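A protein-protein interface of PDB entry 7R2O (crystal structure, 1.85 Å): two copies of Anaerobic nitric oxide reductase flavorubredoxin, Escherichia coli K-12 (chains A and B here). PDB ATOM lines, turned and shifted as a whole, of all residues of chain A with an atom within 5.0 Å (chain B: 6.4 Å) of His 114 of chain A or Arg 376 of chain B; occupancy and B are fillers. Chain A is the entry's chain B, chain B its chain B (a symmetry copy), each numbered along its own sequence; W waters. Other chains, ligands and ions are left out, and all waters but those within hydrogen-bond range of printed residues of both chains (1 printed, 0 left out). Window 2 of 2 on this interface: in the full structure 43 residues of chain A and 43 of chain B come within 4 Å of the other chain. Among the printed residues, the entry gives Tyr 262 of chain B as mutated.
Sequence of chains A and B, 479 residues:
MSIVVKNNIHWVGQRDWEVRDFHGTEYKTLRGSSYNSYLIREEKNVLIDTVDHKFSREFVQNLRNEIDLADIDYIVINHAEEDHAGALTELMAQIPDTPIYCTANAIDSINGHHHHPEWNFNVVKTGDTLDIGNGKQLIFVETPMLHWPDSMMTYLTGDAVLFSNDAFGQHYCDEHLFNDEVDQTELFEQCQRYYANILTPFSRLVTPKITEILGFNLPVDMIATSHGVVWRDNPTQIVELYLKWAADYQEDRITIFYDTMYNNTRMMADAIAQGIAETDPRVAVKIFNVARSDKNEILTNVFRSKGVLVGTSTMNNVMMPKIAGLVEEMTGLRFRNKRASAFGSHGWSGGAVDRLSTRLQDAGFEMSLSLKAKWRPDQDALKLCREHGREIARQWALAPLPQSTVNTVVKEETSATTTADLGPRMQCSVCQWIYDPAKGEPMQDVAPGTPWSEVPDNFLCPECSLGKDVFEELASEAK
No position is printed for both chains.
Of the 9 pairs that touch across the chains among the printed residues, none has its exchanged pair printed and touching as well.
NE of Arg 376 of chain B is in hydrogen-bond range of O of His 113 of chain A (2.9 Å).
A ring nitrogen (NE2) of His 115 of chain A lies close to the backbone carbonyl oxygen (O) of Arg 376 of chain B (3.3 Å).
The backbone NH (N) of Arg 376 of chain B lies within hydrogen-bond range of the backbone carbonyl oxygen (O) of Gly 112 of chain A (3.1 Å).
A ring nitrogen (NE2) of His 115 of chain A sits close to the backbone NH (N) of Asp 378 of chain B (3.5 Å).
His 114 of chain A touches just one residue of chain B: Arg 376.
Of the printed residues of chain A, Arg 376 of chain B touches Gly 112 (3.1 Å), His 113 (2.9 Å), His 114 (3.9 Å) and His 115 (3.0 Å).
Of the printed residues of chain B, Gly 112 of chain A touches Trp 375 (3.4 Å) and Arg 376 (3.1 Å).
Of the printed residues of chain A, Tyr 262 of chain B touches Glu 82 (3.7 Å).
Of the printed residues of chain A, Pro 377 of chain B touches His 115.
Lys 374 of chain B touches none of the printed residues of chain A.
The nearest printed residue of chain A that does not touch Arg 376 of chain B is Asn 111 of chain A (5.8 Å).
Printed residues of chain B that touch a printed residue of chain A: Tyr 262, Trp 375, Arg 376, Pro 377 and Asp 378.
Hydrophobic or aromatic side chains of chain B that line the printed part of chain A: Tyr 262 and Trp 375.
Along chain B the printed residues that touch a printed residue of chain A span positions 262 to 378.
Hydrophobic or aromatic side chains of chain A within 4 Å of the printed part of chain B: His 113 and His 115.
Water W1 lies within hydrogen-bond range of a ring nitrogen (NE2) of His 113 of chain A (2.7 Å) and the side-chain amide nitrogen (ND2) of Asn 264 of chain B (2.8 Å).
CB of Glu 82 of chain A touches CE1 of Tyr 262 of chain B, 3.7 Å away.
Trp 375 of chain B touches Gly 112 of chain A (CB to O, 3.4 Å).
His 113 of chain A touches Trp 375 of chain B.
His 114 of chain A touches Arg 376 of chain B (O to NH2, 3.9 Å).
Pro 377 of chain B touches His 115 of chain A.
OD1 of Asp 378 of chain B lies within hydrogen-bond range of N of Ala 381 of chain B (2.9 Å).
O of His 346 of chain B lies within hydrogen-bond range of N of Trp 375 of chain B, 2.9 Å away.
The backbone carbonyl oxygen of Gly 112 of chain A sits close to a ring nitrogen (ND1) of His 115 of chain A, at 3.5 Å.
O of Ala 85 of chain A sits at hydrogen-bond distance from NE2 of His 114 of chain A.
The backbone carbonyl oxygen (O) of Asn 111 of chain A lies within hydrogen-bond range of a ring nitrogen (ND1) of His 115 of chain A, at 3.0 Å.
The side-chain hydroxyl of Thr 89 of chain A lies within hydrogen-bond range of a ring nitrogen (ND1) of His 114 of chain A, 2.6 Å away.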
ATOM      1  N   GLU A  82      14.447  17.939  16.804  1.00  0.00           N
ATOM      2  CA  GLU A  82      15.037  17.799  15.476  1.00  0.00           C
ATOM      3  C   GLU A  82      14.860  19.039  14.606  1.00  0.00           C
ATOM      4  O   GLU A  82      15.629  19.225  13.658  1.00  0.00           O
ATOM      5  CB  GLU A  82      14.453  16.582  14.762  1.00  0.00           C
ATOM      6  CG  GLU A  82      15.429  15.926  13.802  1.00  0.00           C
ATOM      7  CD  GLU A  82      16.725  15.521  14.484  1.00  0.00           C
ATOM      8  OE1 GLU A  82      16.767  15.526  15.733  1.00  0.00           O
ATOM      9  OE2 GLU A  82      17.701  15.197  13.772  1.00  0.00           O
ATOM     10  N   ALA A  85      18.143  21.117  16.176  1.00  0.00           N
ATOM     11  CA  ALA A  85      19.428  20.436  16.174  1.00  0.00           C
ATOM     12  C   ALA A  85      19.572  19.469  15.009  1.00  0.00           C
ATOM     13  O   ALA A  85      20.496  18.673  15.005  1.00  0.00           O
ATOM     14  CB  ALA A  85      19.640  19.682  17.493  1.00  0.00           C
ATOM     15  N   GLY A  86      18.675  19.512  14.033  1.00  0.00           N
ATOM     16  CA  GLY A  86      18.642  18.474  13.018  1.00  0.00           C
ATOM     17  C   GLY A  86      19.818  18.517  12.083  1.00  0.00           C
ATOM     18  O   GLY A  86      20.150  17.514  11.452  1.00  0.00           O
ATOM     19  N   LEU A  88      22.859  19.250  13.113  1.00  0.00           N
ATOM     20  CA  LEU A  88      24.058  19.188  13.942  1.00  0.00           C
ATOM     21  C   LEU A  88      25.032  18.120  13.450  1.00  0.00           C
ATOM     22  O   LEU A  88      26.246  18.355  13.412  1.00  0.00           O
ATOM     23  CB  LEU A  88      23.658  18.941  15.398  1.00  0.00           C
ATOM     24  CG  LEU A  88      24.717  19.161  16.472  1.00  0.00           C
ATOM     25  CD1 LEU A  88      25.348  20.536  16.321  1.00  0.00           C
ATOM     26  CD2 LEU A  88      24.082  18.996  17.847  1.00  0.00           C
ATOM     27  N   THR A  89      24.530  16.938  13.076  1.00  0.00           N
ATOM     28  CA  THR A  89      25.423  15.884  12.603  1.00  0.00           C
ATOM     29  C   THR A  89      26.204  16.344  11.382  1.00  0.00           C
ATOM     30  O   THR A  89      27.422  16.150  11.296  1.00  0.00           O
ATOM     31  CB  THR A  89      24.639  14.609  12.281  1.00  0.00           C
ATOM     32  OG1 THR A  89      24.225  13.971  13.495  1.00  0.00           O
ATOM     33  CG2 THR A  89      25.508  13.647  11.486  1.00  0.00           C
ATOM     34  N   ILE A 110      20.615  15.167  22.675  1.00  0.00           N
ATOM     35  CA  ILE A 110      21.477  15.261  21.499  1.00  0.00           C
ATOM     36  C   ILE A 110      21.999  13.881  21.116  1.00  0.00           C
ATOM     37  O   ILE A 110      21.880  13.450  19.962  1.00  0.00           O
ATOM     38  CB  ILE A 110      22.631  16.249  21.751  1.00  0.00           C
ATOM     39  CG1 ILE A 110      22.088  17.675  21.904  1.00  0.00           C
ATOM     40  CG2 ILE A 110      23.651  16.159  20.618  1.00  0.00           C
ATOM     41  CD1 ILE A 110      23.142  18.718  22.208  1.00  0.00           C
ATOM     42  N   ASN A 111      22.595  13.169  22.076  1.00  0.00           N
ATOM     43  CA  ASN A 111      23.073  11.817  21.798  1.00  0.00           C
ATOM     44  C   ASN A 111      21.926  10.906  21.384  1.00  0.00           C
ATOM     45  O   ASN A 111      22.095  10.033  20.525  1.00  0.00           O
ATOM     46  CB  ASN A 111      23.787  11.239  23.021  1.00  0.00           C
ATOM     47  CG  ASN A 111      25.155  11.852  23.249  1.00  0.00           C
ATOM     48  OD1 ASN A 111      25.814  12.309  22.314  1.00  0.00           O
ATOM     49  ND2 ASN A 111      25.593  11.854  24.500  1.00  0.00           N
ATOM     50  N   GLY A 112      20.752  11.094  21.988  1.00  0.00           N
ATOM     51  CA  GLY A 112      19.611  10.262  21.645  1.00  0.00           C
ATOM     52  C   GLY A 112      19.287  10.294  20.165  1.00  0.00           C
ATOM     53  O   GLY A 112      18.934   9.270  19.577  1.00  0.00           O
ATOM     54  N   HIS A 113      19.411  11.466  19.539  1.00  0.00           N
ATOM     55  CA  HIS A 113      19.131  11.610  18.114  1.00  0.00           C
ATOM     56  C   HIS A 113      20.360  11.344  17.248  1.00  0.00           C
ATOM     57  O   HIS A 113      20.271  10.629  16.246  1.00  0.00           O
ATOM     58  CB  HIS A 113      18.585  13.012  17.818  1.00  0.00           C
ATOM     59  CG  HIS A 113      17.242  13.282  18.421  1.00  0.00           C
ATOM     60  ND1 HIS A 113      17.084  13.938  19.622  1.00  0.00           N
ATOM     61  CD2 HIS A 113      15.993  12.986  17.988  1.00  0.00           C
ATOM     62  CE1 HIS A 113      15.797  14.037  19.902  1.00  0.00           C
ATOM     63  NE2 HIS A 113      15.113  13.467  18.927  1.00  0.00           N
ATOM     64  N   HIS A 114      21.513  11.896  17.628  1.00  0.00           N
ATOM     65  CA  HIS A 114      22.664  11.951  16.734  1.00  0.00           C
ATOM     66  C   HIS A 114      23.649  10.804  16.926  1.00  0.00           C
ATOM     67  O   HIS A 114      24.371  10.459  15.982  1.00  0.00           O
ATOM     68  CB  HIS A 114      23.378  13.293  16.909  1.00  0.00           C
ATOM     69  CG  HIS A 114      22.536  14.463  16.514  1.00  0.00           C
ATOM     70  ND1 HIS A 114      22.489  14.942  15.222  1.00  0.00           N
ATOM     71  CD2 HIS A 114      21.681  15.230  17.231  1.00  0.00           C
ATOM     72  CE1 HIS A 114      21.655  15.964  15.163  1.00  0.00           C
ATOM     73  NE2 HIS A 114      21.152  16.160  16.370  1.00  0.00           N
ATOM     74  N   HIS A 115      23.703  10.208  18.116  1.00  0.00           N
ATOM     75  CA  HIS A 115      24.539   9.039  18.375  1.00  0.00           C
ATOM     76  C   HIS A 115      26.030   9.361  18.304  1.00  0.00           C
ATOM     77  O   HIS A 115      26.836   8.496  17.958  1.00  0.00           O
ATOM     78  CB  HIS A 115      24.222   7.895  17.407  1.00  0.00           C
ATOM     79  CG  HIS A 115      22.804   7.415  17.461  1.00  0.00           C
ATOM     80  ND1 HIS A 115      21.894   7.874  18.389  1.00  0.00           N
ATOM     81  CD2 HIS A 115      22.143   6.513  16.697  1.00  0.00           C
ATOM     82  CE1 HIS A 115      20.733   7.275  18.194  1.00  0.00           C
ATOM     83  NE2 HIS A 115      20.856   6.443  17.175  1.00  0.00           N
ATOM     84  N   HIS A 116      26.423  10.595  18.613  1.00  0.00           N
ATOM     85  CA  HIS A 116      27.827  11.003  18.600  1.00  0.00           C
ATOM     86  C   HIS A 116      28.217  11.501  19.987  1.00  0.00           C
ATOM     87  O   HIS A 116      28.461  12.697  20.192  1.00  0.00           O
ATOM     88  CB  HIS A 116      28.087  12.070  17.540  1.00  0.00           C
ATOM     89  CG  HIS A 116      28.118  11.531  16.144  1.00  0.00           C
ATOM     90  ND1 HIS A 116      29.243  10.957  15.594  1.00  0.00           N
ATOM     91  CD2 HIS A 116      27.160  11.472  15.189  1.00  0.00           C
ATOM     92  CE1 HIS A 116      28.980  10.572  14.358  1.00  0.00           C
ATOM     93  NE2 HIS A 116      27.722  10.873  14.087  1.00  0.00           N
ATOM     94  N   TRP A 119      31.374  13.832  20.857  1.00  0.00           N
ATOM     95  CA  TRP A 119      31.357  15.284  20.740  1.00  0.00           C
ATOM     96  C   TRP A 119      31.739  15.932  22.069  1.00  0.00           C
ATOM     97  O   TRP A 119      31.606  15.312  23.132  1.00  0.00           O
ATOM     98  CB  TRP A 119      29.982  15.765  20.279  1.00  0.00           C
ATOM     99  CG  TRP A 119      29.691  15.470  18.830  1.00  0.00           C
ATOM    100  CD1 TRP A 119      30.583  15.062  17.878  1.00  0.00           C
ATOM    101  CD2 TRP A 119      28.417  15.561  18.172  1.00  0.00           C
ATOM    102  NE1 TRP A 119      29.945  14.894  16.670  1.00  0.00           N
ATOM    103  CE2 TRP A 119      28.617  15.196  16.824  1.00  0.00           C
ATOM    104  CE3 TRP A 119      27.131  15.918  18.593  1.00  0.00           C
ATOM    105  CZ2 TRP A 119      27.575  15.171  15.894  1.00  0.00           C
ATOM    106  CZ3 TRP A 119      26.097  15.897  17.668  1.00  0.00           C
ATOM    107  CH2 TRP A 119      26.327  15.526  16.333  1.00  0.00           C
ATOM    108  N   TYR B 262       8.837  11.752  14.800  1.00  0.00           N
ATOM    109  CA  TYR B 262      10.154  11.901  14.196  1.00  0.00           C
ATOM    110  C   TYR B 262      10.675  10.588  13.624  1.00  0.00           C
ATOM    111  O   TYR B 262      11.875  10.462  13.360  1.00  0.00           O
ATOM    112  CB  TYR B 262      11.133  12.491  15.211  1.00  0.00           C
ATOM    113  CG  TYR B 262      10.776  13.915  15.567  1.00  0.00           C
ATOM    114  CD1 TYR B 262      11.071  14.958  14.701  1.00  0.00           C
ATOM    115  CD2 TYR B 262      10.123  14.216  16.758  1.00  0.00           C
ATOM    116  CE1 TYR B 262      10.738  16.259  15.014  1.00  0.00           C
ATOM    117  CE2 TYR B 262       9.786  15.518  17.080  1.00  0.00           C
ATOM    118  CZ  TYR B 262      10.095  16.535  16.204  1.00  0.00           C
ATOM    119  OH  TYR B 262       9.764  17.836  16.507  1.00  0.00           O
ATOM    120  N   ASN B 264      11.038   7.700  14.942  1.00  0.00           N
ATOM    121  CA  ASN B 264      11.698   6.761  15.840  1.00  0.00           C
ATOM    122  C   ASN B 264      10.861   5.502  16.018  1.00  0.00           C
ATOM    123  O   ASN B 264      11.366   4.381  15.882  1.00  0.00           O
ATOM    124  CB  ASN B 264      11.977   7.432  17.185  1.00  0.00           C
ATOM    125  CG  ASN B 264      12.926   8.607  17.056  1.00  0.00           C
ATOM    126  OD1 ASN B 264      13.863   8.573  16.258  1.00  0.00           O
ATOM    127  ND2 ASN B 264      12.682   9.659  17.832  1.00  0.00           N
ATOM    128  N   MET B 267      11.064   3.397  12.914  1.00  0.00           N
ATOM    129  CA  MET B 267      12.261   2.567  12.850  1.00  0.00           C
ATOM    130  C   MET B 267      12.091   1.293  13.666  1.00  0.00           C
ATOM    131  O   MET B 267      12.558   0.220  13.259  1.00  0.00           O
ATOM    132  CB  MET B 267      13.475   3.362  13.334  1.00  0.00           C
ATOM    133  CG  MET B 267      13.928   4.431  12.355  1.00  0.00           C
ATOM    134  SD  MET B 267      15.199   5.526  13.018  1.00  0.00           S
ATOM    135  CE  MET B 267      16.602   4.420  13.127  1.00  0.00           C
ATOM    136  N   SER B 345       8.618   4.802  20.994  1.00  0.00           N
ATOM    137  CA  SER B 345       9.749   5.586  21.460  1.00  0.00           C
ATOM    138  C   SER B 345       9.269   6.704  22.379  1.00  0.00           C
ATOM    139  O   SER B 345       8.140   7.184  22.265  1.00  0.00           O
ATOM    140  CB  SER B 345      10.521   6.174  20.272  1.00  0.00           C
ATOM    141  OG  SER B 345      11.562   7.038  20.696  1.00  0.00           O
ATOM    142  N   HIS B 346      10.141   7.116  23.294  1.00  0.00           N
ATOM    143  CA  HIS B 346       9.840   8.189  24.229  1.00  0.00           C
ATOM    144  C   HIS B 346      11.087   9.039  24.415  1.00  0.00           C
ATOM    145  O   HIS B 346      12.197   8.640  24.052  1.00  0.00           O
ATOM    146  CB  HIS B 346       9.369   7.646  25.580  1.00  0.00           C
ATOM    147  CG  HIS B 346      10.398   6.808  26.272  1.00  0.00           C
ATOM    148  ND1 HIS B 346      10.376   5.431  26.250  1.00  0.00           N
ATOM    149  CD2 HIS B 346      11.493   7.156  26.989  1.00  0.00           C
ATOM    150  CE1 HIS B 346      11.408   4.965  26.931  1.00  0.00           C
ATOM    151  NE2 HIS B 346      12.102   5.991  27.389  1.00  0.00           N
ATOM    152  N   ALA B 373      11.911   2.126  23.487  1.00  0.00           N
ATOM    153  CA  ALA B 373      13.221   2.664  23.158  1.00  0.00           C
ATOM    154  C   ALA B 373      13.211   4.161  23.431  1.00  0.00           C
ATOM    155  O   ALA B 373      12.164   4.810  23.376  1.00  0.00           O
ATOM    156  CB  ALA B 373      13.606   2.379  21.700  1.00  0.00           C
ATOM    157  N   LYS B 374      14.387   4.699  23.732  1.00  0.00           N
ATOM    158  CA  LYS B 374      14.547   6.116  24.019  1.00  0.00           C
ATOM    159  C   LYS B 374      15.078   6.825  22.779  1.00  0.00           C
ATOM    160  O   LYS B 374      16.051   6.368  22.167  1.00  0.00           O
ATOM    161  CB  LYS B 374      15.492   6.310  25.205  1.00  0.00           C
ATOM    162  CG  LYS B 374      15.375   7.652  25.903  1.00  0.00           C
ATOM    163  CD  LYS B 374      16.377   7.751  27.043  1.00  0.00           C
ATOM    164  CE  LYS B 374      16.221   9.048  27.805  1.00  0.00           C
ATOM    165  NZ  LYS B 374      17.141   9.119  28.970  1.00  0.00           N
ATOM    166  N   TRP B 375      14.434   7.933  22.404  1.00  0.00           N
ATOM    167  CA  TRP B 375      14.844   8.723  21.245  1.00  0.00           C
ATOM    168  C   TRP B 375      15.021   7.843  20.010  1.00  0.00           C
ATOM    169  O   TRP B 375      14.226   6.926  19.781  1.00  0.00           O
ATOM    170  CB  TRP B 375      16.139   9.494  21.540  1.00  0.00           C
ATOM    171  CG  TRP B 375      16.058  10.411  22.736  1.00  0.00           C
ATOM    172  CD1 TRP B 375      16.818  10.345  23.865  1.00  0.00           C
ATOM    173  CD2 TRP B 375      15.161  11.521  22.920  1.00  0.00           C
ATOM    174  NE1 TRP B 375      16.457  11.345  24.739  1.00  0.00           N
ATOM    175  CE2 TRP B 375      15.445  12.082  24.183  1.00  0.00           C
ATOM    176  CE3 TRP B 375      14.153  12.095  22.141  1.00  0.00           C
ATOM    177  CZ2 TRP B 375      14.755  13.189  24.685  1.00  0.00           C
ATOM    178  CZ3 TRP B 375      13.465  13.194  22.641  1.00  0.00           C
ATOM    179  CH2 TRP B 375      13.771  13.728  23.900  1.00  0.00           C
ATOM    180  N   ARG B 376      16.071   8.113  19.197  1.00  0.00           N
ATOM    181  CA  ARG B 376      16.239   7.306  17.990  1.00  0.00           C
ATOM    182  C   ARG B 376      17.012   6.035  18.315  1.00  0.00           C
ATOM    183  O   ARG B 376      18.081   6.110  18.932  1.00  0.00           O
ATOM    184  CB  ARG B 376      16.965   8.080  16.895  1.00  0.00           C
ATOM    185  CG  ARG B 376      17.186   7.261  15.616  1.00  0.00           C
ATOM    186  CD  ARG B 376      17.632   8.110  14.422  1.00  0.00           C
ATOM    187  NE  ARG B 376      18.977   8.658  14.583  1.00  0.00           N
ATOM    188  CZ  ARG B 376      20.097   8.022  14.238  1.00  0.00           C
ATOM    189  NH1 ARG B 376      20.034   6.802  13.714  1.00  0.00           N
ATOM    190  NH2 ARG B 376      21.281   8.605  14.416  1.00  0.00           N
ATOM    191  N   PRO B 377      16.509   4.865  17.920  1.00  0.00           N
ATOM    192  CA  PRO B 377      17.220   3.607  18.199  1.00  0.00           C
ATOM    193  C   PRO B 377      18.537   3.552  17.442  1.00  0.00           C
ATOM    194  O   PRO B 377      18.561   3.661  16.215  1.00  0.00           O
ATOM    195  CB  PRO B 377      16.247   2.528  17.705  1.00  0.00           C
ATOM    196  CG  PRO B 377      14.919   3.207  17.620  1.00  0.00           C
ATOM    197  CD  PRO B 377      15.202   4.635  17.283  1.00  0.00           C
ATOM    198  N   ASP B 378      19.633   3.371  18.173  1.00  0.00           N
ATOM    199  CA  ASP B 378      20.921   3.134  17.539  1.00  0.00           C
ATOM    200  C   ASP B 378      20.999   1.655  17.151  1.00  0.00           C
ATOM    201  O   ASP B 378      20.023   0.908  17.264  1.00  0.00           O
ATOM    202  CB  ASP B 378      22.061   3.582  18.454  1.00  0.00           C
ATOM    203  CG  ASP B 378      22.148   2.772  19.731  1.00  0.00           C
ATOM    204  OD1 ASP B 378      21.318   1.861  19.929  1.00  0.00           O
ATOM    205  OD2 ASP B 378      23.059   3.049  20.540  1.00  0.00           O
ATOM    206  N   GLN B 379      22.166   1.211  16.679  1.00  0.00           N
ATOM    207  CA  GLN B 379      22.274  -0.159  16.189  1.00  0.00           C
ATOM    208  C   GLN B 379      21.956  -1.169  17.284  1.00  0.00           C
ATOM    209  O   GLN B 379      21.332  -2.204  17.019  1.00  0.00           O
ATOM    210  CB  GLN B 379      23.667  -0.404  15.610  1.00  0.00           C
ATOM    211  CG  GLN B 379      23.896   0.300  14.287  1.00  0.00           C
ATOM    212  CD  GLN B 379      22.771   0.049  13.301  1.00  0.00           C
ATOM    213  OE1 GLN B 379      22.458  -1.097  12.976  1.00  0.00           O
ATOM    214  NE2 GLN B 379      22.148   1.123  12.828  1.00  0.00           N
ATOM    215  N   ALA B 381      19.883  -0.709  19.891  1.00  0.00           N
ATOM    216  CA  ALA B 381      18.448  -0.707  20.153  1.00  0.00           C
ATOM    217  C   ALA B 381      17.682  -1.410  19.039  1.00  0.00           C
ATOM    218  O   ALA B 381      16.706  -2.122  19.302  1.00  0.00           O
ATOM    219  CB  ALA B 381      17.947   0.727  20.332  1.00  0.00           C
HETATM  220  O   HOH W   1      12.730  12.213  19.003  1.00  0.00           O
